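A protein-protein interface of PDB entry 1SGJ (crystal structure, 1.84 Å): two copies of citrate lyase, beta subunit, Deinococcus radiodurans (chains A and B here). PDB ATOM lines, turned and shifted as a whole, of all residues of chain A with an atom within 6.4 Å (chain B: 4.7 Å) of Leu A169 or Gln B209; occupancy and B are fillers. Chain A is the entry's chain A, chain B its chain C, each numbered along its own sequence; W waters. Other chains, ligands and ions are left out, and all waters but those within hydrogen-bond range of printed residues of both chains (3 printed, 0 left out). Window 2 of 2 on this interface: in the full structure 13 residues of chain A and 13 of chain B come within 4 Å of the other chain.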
ATOM      1  N   ARG A 164     -31.406   0.139  14.973  1.00  0.00           N
ATOM      2  CA  ARG A 164     -31.094   0.128  13.547  1.00  0.00           C
ATOM      3  C   ARG A 164     -29.696   0.642  13.186  1.00  0.00           C
ATOM      4  O   ARG A 164     -29.180   1.571  13.806  1.00  0.00           O
ATOM      5  CB  ARG A 164     -32.152   0.945  12.796  1.00  0.00           C
ATOM      6  CG  ARG A 164     -33.532   0.291  12.761  1.00  0.00           C
ATOM      7  CD  ARG A 164     -33.630  -0.702  11.616  1.00  0.00           C
ATOM      8  NE  ARG A 164     -33.741  -0.028  10.320  1.00  0.00           N
ATOM      9  CZ  ARG A 164     -32.980  -0.307   9.266  1.00  0.00           C
ATOM     10  NH1 ARG A 164     -32.049  -1.243   9.350  1.00  0.00           N
ATOM     11  NH2 ARG A 164     -33.151   0.346   8.125  1.00  0.00           N
ATOM     12  N   THR A 165     -29.090   0.024  12.175  1.00  0.00           N
ATOM     13  CA  THR A 165     -27.770   0.430  11.698  1.00  0.00           C
ATOM     14  C   THR A 165     -27.860   0.640  10.186  1.00  0.00           C
ATOM     15  O   THR A 165     -28.804   0.172   9.544  1.00  0.00           O
ATOM     16  CB  THR A 165     -26.703  -0.647  11.968  1.00  0.00           C
ATOM     17  OG1 THR A 165     -26.931  -1.774  11.110  1.00  0.00           O
ATOM     18  CG2 THR A 165     -26.750  -1.093  13.423  1.00  0.00           C
ATOM     19  N   PRO A 166     -26.889   1.352   9.598  1.00  0.00           N
ATOM     20  CA  PRO A 166     -26.914   1.586   8.150  1.00  0.00           C
ATOM     21  C   PRO A 166     -26.847   0.279   7.350  1.00  0.00           C
ATOM     22  O   PRO A 166     -27.571   0.100   6.373  1.00  0.00           O
ATOM     23  CB  PRO A 166     -25.685   2.468   7.927  1.00  0.00           C
ATOM     24  CG  PRO A 166     -25.607   3.256   9.199  1.00  0.00           C
ATOM     25  CD  PRO A 166     -25.858   2.185  10.245  1.00  0.00           C
ATOM     26  N   GLY A 167     -25.967  -0.626   7.771  1.00  0.00           N
ATOM     27  CA  GLY A 167     -25.818  -1.901   7.094  1.00  0.00           C
ATOM     28  C   GLY A 167     -27.073  -2.754   7.171  1.00  0.00           C
ATOM     29  O   GLY A 167     -27.402  -3.473   6.230  1.00  0.00           O
ATOM     30  N   GLY A 168     -27.773  -2.678   8.300  1.00  0.00           N
ATOM     31  CA  GLY A 168     -28.998  -3.439   8.464  1.00  0.00           C
ATOM     32  C   GLY A 168     -28.810  -4.921   8.746  1.00  0.00           C
ATOM     33  O   GLY A 168     -29.746  -5.705   8.578  1.00  0.00           O
ATOM     34  N   LEU A 169     -27.615  -5.320   9.176  1.00  0.00           N
ATOM     35  CA  LEU A 169     -27.385  -6.728   9.477  1.00  0.00           C
ATOM     36  C   LEU A 169     -28.343  -7.197  10.570  1.00  0.00           C
ATOM     37  O   LEU A 169     -28.683  -8.380  10.635  1.00  0.00           O
ATOM     38  CB  LEU A 169     -25.940  -6.972   9.928  1.00  0.00           C
ATOM     39  CG  LEU A 169     -24.829  -6.886   8.871  1.00  0.00           C
ATOM     40  CD1 LEU A 169     -23.505  -7.278   9.514  1.00  0.00           C
ATOM     41  CD2 LEU A 169     -25.140  -7.813   7.688  1.00  0.00           C
ATOM     42  N   GLU A 170     -28.788  -6.270  11.417  1.00  0.00           N
ATOM     43  CA  GLU A 170     -29.695  -6.614  12.503  1.00  0.00           C
ATOM     44  C   GLU A 170     -31.103  -6.980  12.029  1.00  0.00           C
ATOM     45  O   GLU A 170     -31.890  -7.514  12.798  1.00  0.00           O
ATOM     46  CB  GLU A 170     -29.766  -5.481  13.541  1.00  0.00           C
ATOM     47  CG  GLU A 170     -30.577  -4.252  13.147  1.00  0.00           C
ATOM     48  CD  GLU A 170     -29.870  -3.346  12.157  1.00  0.00           C
ATOM     49  OE1 GLU A 170     -28.636  -3.469  11.998  1.00  0.00           O
ATOM     50  OE2 GLU A 170     -30.553  -2.494  11.545  1.00  0.00           O
ATOM     51  N   VAL A 171     -31.428  -6.690  10.770  1.00  0.00           N
ATOM     52  CA  VAL A 171     -32.741  -7.050  10.246  1.00  0.00           C
ATOM     53  C   VAL A 171     -32.615  -7.923   9.010  1.00  0.00           C
ATOM     54  O   VAL A 171     -33.606  -8.219   8.365  1.00  0.00           O
ATOM     55  CB  VAL A 171     -33.607  -5.812   9.891  1.00  0.00           C
ATOM     56  CG1 VAL A 171     -33.834  -4.964  11.138  1.00  0.00           C
ATOM     57  CG2 VAL A 171     -32.944  -4.994   8.783  1.00  0.00           C
ATOM     58  N   LEU A 172     -31.397  -8.357   8.691  1.00  0.00           N
ATOM     59  CA  LEU A 172     -31.185  -9.195   7.511  1.00  0.00           C
ATOM     60  C   LEU A 172     -31.984 -10.495   7.553  1.00  0.00           C
ATOM     61  O   LEU A 172     -32.549 -10.918   6.547  1.00  0.00           O
ATOM     62  CB  LEU A 172     -29.702  -9.529   7.342  1.00  0.00           C
ATOM     63  CG  LEU A 172     -29.369 -10.398   6.124  1.00  0.00           C
ATOM     64  CD1 LEU A 172     -29.848  -9.696   4.857  1.00  0.00           C
ATOM     65  CD2 LEU A 172     -27.850 -10.632   6.050  1.00  0.00           C
ATOM     66  N   TYR A 173     -32.014 -11.135   8.714  1.00  0.00           N
ATOM     67  CA  TYR A 173     -32.757 -12.379   8.878  1.00  0.00           C
ATOM     68  C   TYR A 173     -34.231 -12.126   8.532  1.00  0.00           C
ATOM     69  O   TYR A 173     -34.810 -12.808   7.698  1.00  0.00           O
ATOM     70  CB  TYR A 173     -32.616 -12.847  10.327  1.00  0.00           C
ATOM     71  CG  TYR A 173     -33.533 -13.974  10.742  1.00  0.00           C
ATOM     72  CD1 TYR A 173     -33.151 -15.302  10.597  1.00  0.00           C
ATOM     73  CD2 TYR A 173     -34.778 -13.702  11.319  1.00  0.00           C
ATOM     74  CE1 TYR A 173     -33.978 -16.348  11.023  1.00  0.00           C
ATOM     75  CE2 TYR A 173     -35.617 -14.732  11.743  1.00  0.00           C
ATOM     76  CZ  TYR A 173     -35.209 -16.052  11.596  1.00  0.00           C
ATOM     77  OH  TYR A 173     -36.022 -17.073  12.032  1.00  0.00           O
ATOM     78  N   GLN A 209     -29.467  -3.574  -1.692  1.00  0.00           N
ATOM     79  CA  GLN A 209     -29.562  -4.743  -0.820  1.00  0.00           C
ATOM     80  C   GLN A 209     -30.961  -5.355  -0.936  1.00  0.00           C
ATOM     81  O   GLN A 209     -31.107  -6.576  -1.016  1.00  0.00           O
ATOM     82  CB  GLN A 209     -29.302  -4.339   0.632  1.00  0.00           C
ATOM     83  CG  GLN A 209     -29.499  -5.469   1.649  1.00  0.00           C
ATOM     84  CD  GLN A 209     -28.568  -6.658   1.419  1.00  0.00           C
ATOM     85  OE1 GLN A 209     -28.776  -7.474   0.503  1.00  0.00           O
ATOM     86  NE2 GLN A 209     -27.533  -6.759   2.250  1.00  0.00           N
ATOM     87  N   LEU B 169     -20.845 -13.506  10.850  1.00  0.00           N
ATOM     88  CA  LEU B 169     -21.904 -13.708   9.863  1.00  0.00           C
ATOM     89  C   LEU B 169     -22.349 -15.164   9.829  1.00  0.00           C
ATOM     90  O   LEU B 169     -23.476 -15.469   9.432  1.00  0.00           O
ATOM     91  CB  LEU B 169     -21.436 -13.310   8.461  1.00  0.00           C
ATOM     92  CG  LEU B 169     -21.175 -11.835   8.152  1.00  0.00           C
ATOM     93  CD1 LEU B 169     -20.693 -11.714   6.715  1.00  0.00           C
ATOM     94  CD2 LEU B 169     -22.449 -11.016   8.363  1.00  0.00           C
ATOM     95  N   LEU B 172     -25.192 -15.345  12.266  1.00  0.00           N
ATOM     96  CA  LEU B 172     -26.149 -14.244  12.230  1.00  0.00           C
ATOM     97  C   LEU B 172     -27.587 -14.755  12.166  1.00  0.00           C
ATOM     98  O   LEU B 172     -28.465 -14.232  12.846  1.00  0.00           O
ATOM     99  CB  LEU B 172     -25.873 -13.324  11.034  1.00  0.00           C
ATOM    100  CG  LEU B 172     -26.857 -12.162  10.857  1.00  0.00           C
ATOM    101  CD1 LEU B 172     -26.953 -11.351  12.147  1.00  0.00           C
ATOM    102  CD2 LEU B 172     -26.392 -11.275   9.717  1.00  0.00           C
ATOM    103  N   ARG B 175     -28.330 -16.201  15.638  1.00  0.00           N
ATOM    104  CA  ARG B 175     -28.459 -15.148  16.641  1.00  0.00           C
ATOM    105  C   ARG B 175     -29.748 -14.339  16.439  1.00  0.00           C
ATOM    106  O   ARG B 175     -30.393 -13.925  17.406  1.00  0.00           O
ATOM    107  CB  ARG B 175     -27.249 -14.197  16.606  1.00  0.00           C
ATOM    108  CG  ARG B 175     -26.806 -13.774  18.012  1.00  0.00           C
ATOM    109  CD  ARG B 175     -26.109 -12.413  18.131  1.00  0.00           C
ATOM    110  NE  ARG B 175     -24.912 -12.283  17.317  1.00  0.00           N
ATOM    111  CZ  ARG B 175     -23.902 -11.450  17.572  1.00  0.00           C
ATOM    112  NH1 ARG B 175     -23.914 -10.659  18.638  1.00  0.00           N
ATOM    113  NH2 ARG B 175     -22.879 -11.390  16.732  1.00  0.00           N
ATOM    114  N   ALA B 205     -17.715  -3.630  19.658  1.00  0.00           N
ATOM    115  CA  ALA B 205     -18.347  -3.815  18.359  1.00  0.00           C
ATOM    116  C   ALA B 205     -19.272  -5.031  18.366  1.00  0.00           C
ATOM    117  O   ALA B 205     -20.330  -5.023  17.731  1.00  0.00           O
ATOM    118  CB  ALA B 205     -17.282  -3.978  17.286  1.00  0.00           C
ATOM    119  N   ASP B 206     -18.865  -6.070  19.092  1.00  0.00           N
ATOM    120  CA  ASP B 206     -19.639  -7.301  19.192  1.00  0.00           C
ATOM    121  C   ASP B 206     -20.915  -7.060  19.995  1.00  0.00           C
ATOM    122  O   ASP B 206     -21.992  -7.531  19.622  1.00  0.00           O
ATOM    123  CB  ASP B 206     -18.797  -8.387  19.863  1.00  0.00           C
ATOM    124  CG  ASP B 206     -19.445  -9.752  19.803  1.00  0.00           C
ATOM    125  OD1 ASP B 206     -18.813 -10.682  19.258  1.00  0.00           O
ATOM    126  OD2 ASP B 206     -20.577  -9.908  20.303  1.00  0.00           O
ATOM    127  N   ALA B 207     -20.780  -6.322  21.094  1.00  0.00           N
ATOM    128  CA  ALA B 207     -21.904  -5.997  21.959  1.00  0.00           C
ATOM    129  C   ALA B 207     -22.914  -5.137  21.208  1.00  0.00           C
ATOM    130  O   ALA B 207     -24.127  -5.280  21.378  1.00  0.00           O
ATOM    131  CB  ALA B 207     -21.411  -5.256  23.191  1.00  0.00           C
ATOM    132  N   GLU B 208     -22.405  -4.231  20.381  1.00  0.00           N
ATOM    133  CA  GLU B 208     -23.262  -3.352  19.603  1.00  0.00           C
ATOM    134  C   GLU B 208     -24.112  -4.165  18.623  1.00  0.00           C
ATOM    135  O   GLU B 208     -25.258  -3.815  18.342  1.00  0.00           O
ATOM    136  CB  GLU B 208     -22.414  -2.335  18.845  1.00  0.00           C
ATOM    137  CG  GLU B 208     -23.222  -1.305  18.088  1.00  0.00           C
ATOM    138  CD  GLU B 208     -22.377  -0.130  17.657  1.00  0.00           C
ATOM    139  OE1 GLU B 208     -21.430  -0.333  16.866  1.00  0.00           O
ATOM    140  OE2 GLU B 208     -22.656   0.997  18.115  1.00  0.00           O
ATOM    141  N   GLN B 209     -23.548  -5.248  18.100  1.00  0.00           N
ATOM    142  CA  GLN B 209     -24.281  -6.091  17.167  1.00  0.00           C
ATOM    143  C   GLN B 209     -25.404  -6.802  17.924  1.00  0.00           C
ATOM    144  O   GLN B 209     -26.541  -6.864  17.443  1.00  0.00           O
ATOM    145  CB  GLN B 209     -23.343  -7.114  16.523  1.00  0.00           C
ATOM    146  CG  GLN B 209     -24.028  -8.094  15.580  1.00  0.00           C
ATOM    147  CD  GLN B 209     -24.676  -7.421  14.380  1.00  0.00           C
ATOM    148  OE1 GLN B 209     -25.693  -6.723  14.508  1.00  0.00           O
ATOM    149  NE2 GLN B 209     -24.088  -7.630  13.197  1.00  0.00           N
ATOM    150  N   GLY B 210     -25.082  -7.319  19.110  1.00  0.00           N
ATOM    151  CA  GLY B 210     -26.072  -8.014  19.913  1.00  0.00           C
ATOM    152  C   GLY B 210     -27.212  -7.102  20.321  1.00  0.00           C
ATOM    153  O   GLY B 210     -28.381  -7.478  20.261  1.00  0.00           O
ATOM    154  N   ARG B 211     -26.865  -5.889  20.733  1.00  0.00           N
ATOM    155  CA  ARG B 211     -27.857  -4.912  21.146  1.00  0.00           C
ATOM    156  C   ARG B 211     -28.794  -4.596  19.984  1.00  0.00           C
ATOM    157  O   ARG B 211     -30.012  -4.599  20.136  1.00  0.00           O
ATOM    158  CB  ARG B 211     -27.161  -3.629  21.602  1.00  0.00           C
ATOM    159  CG  ARG B 211     -28.102  -2.543  22.068  1.00  0.00           C
ATOM    160  CD  ARG B 211     -28.756  -2.922  23.381  1.00  0.00           C
ATOM    161  NE  ARG B 211     -29.625  -1.858  23.876  1.00  0.00           N
ATOM    162  CZ  ARG B 211     -30.755  -1.491  23.283  1.00  0.00           C
ATOM    163  NH1 ARG B 211     -31.151  -2.102  22.176  1.00  0.00           N
ATOM    164  NH2 ARG B 211     -31.491  -0.520  23.800  1.00  0.00           N
ATOM    165  N   ALA B 212     -28.216  -4.327  18.818  1.00  0.00           N
ATOM    166  CA  ALA B 212     -29.015  -3.997  17.644  1.00  0.00           C
ATOM    167  C   ALA B 212     -30.015  -5.108  17.292  1.00  0.00           C
ATOM    168  O   ALA B 212     -31.132  -4.822  16.864  1.00  0.00           O
ATOM    169  CB  ALA B 212     -28.099  -3.699  16.453  1.00  0.00           C
ATOM    170  N   LEU B 213     -29.615  -6.364  17.498  1.00  0.00           N
ATOM    171  CA  LEU B 213     -30.468  -7.523  17.205  1.00  0.00           C
ATOM    172  C   LEU B 213     -31.609  -7.789  18.187  1.00  0.00           C
ATOM    173  O   LEU B 213     -32.459  -8.642  17.931  1.00  0.00           O
ATOM    174  CB  LEU B 213     -29.618  -8.795  17.105  1.00  0.00           C
ATOM    175  CG  LEU B 213     -28.817  -9.009  15.816  1.00  0.00           C
ATOM    176  CD1 LEU B 213     -27.755 -10.070  16.042  1.00  0.00           C
ATOM    177  CD2 LEU B 213     -29.752  -9.427  14.695  1.00  0.00           C
HETATM  178  O   HOH W   1     -26.025  -4.469  13.292  1.00  0.00           O
HETATM  179  O   HOH W   2     -33.262  -6.042  15.481  1.00  0.00           O
HETATM  180  O   HOH W   3     -33.435  -8.587  15.328  1.00  0.00           O
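OE2 of Glu A170 lies within salt-bridge range of NH1 of Arg A164 (2.9 Å). OE1 of Glu A170 sits at hydrogen-bond distance from OG1 of Thr A165.
Leu B172 touches Leu A169. NE2 of Gln B209 touches CD1 of Leu A169 (3.7 Å). CB of Glu A170 touches O of Ala B212, at 3.7 Å. Leu B213 touches Glu A170. Leu A172 touches Leu B172 (CD2 to CD2, 3.998 Å).
Of chain B, only Leu B172 and Gln B209 come within 4 Å of Leu A169. Gln B209 touches one residue of chain A. Of the printed residues of chain A, Leu B172 touches Leu A169 and Leu A172. Of the printed residues of chain A, Ala B212 touches Glu A170. Of the printed residues of chain B, Glu A170 touches Ala B212 (3.7 Å) and Leu B213 (3.4 Å). Of the printed residues of chain A, Leu B213 touches Glu A170 (3.4 Å). Printed residues of chain B within 4 Å of Leu A172: Leu B172 (3.998 Å). Arg A164 touches none of the printed residues of chain B. The nearest residue of chain B that does not touch Leu A169 is Leu B169 (4.1 Å). The nearest printed residue of chain A that does not touch Leu B172 is Tyr A173 (5.0 Å).
Of the 12 printed residues of chain B, 4 touch a printed residue of chain A. Hydrophobic or aromatic side chains of chain B within 4 Å of the printed part of chain A: Leu B172, Ala B212 and Leu B213. Hydrophobic or aromatic side chains of chain A within 4 Å of the printed part of chain B: Leu A169 and Leu A172. Among the printed residues, 5 pairs touch across the chains.
Leu A169 touches Leu B172, but with the chains exchanged Leu A172 does not touch Leu B169 (5.9 Å). Leu A169 touches Gln B209, but with the chains exchanged Gln A209 does not touch Leu B169 (9.0 Å). Leu A172 touches its own counterpart, Leu B172. Of the 5 pairs that touch across the chains among the printed residues, 1 has its exchanged pair printed and touching as well.
Water W1 bridges OE1 of Gln B209 (2.6 Å) and OE1 of Glu A170 (3.1 Å). Water W3 lies within hydrogen-bond range of the backbone carbonyl oxygen (O) of Leu B213 (2.8 Å) and the backbone carbonyl oxygen (O) of Glu A170 (3.2 Å). Water W2 lies within hydrogen-bond range of the backbone carbonyl oxygen of Ala B212 (2.8 Å) and the backbone carbonyl oxygen of Glu A170 (3.4 Å).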
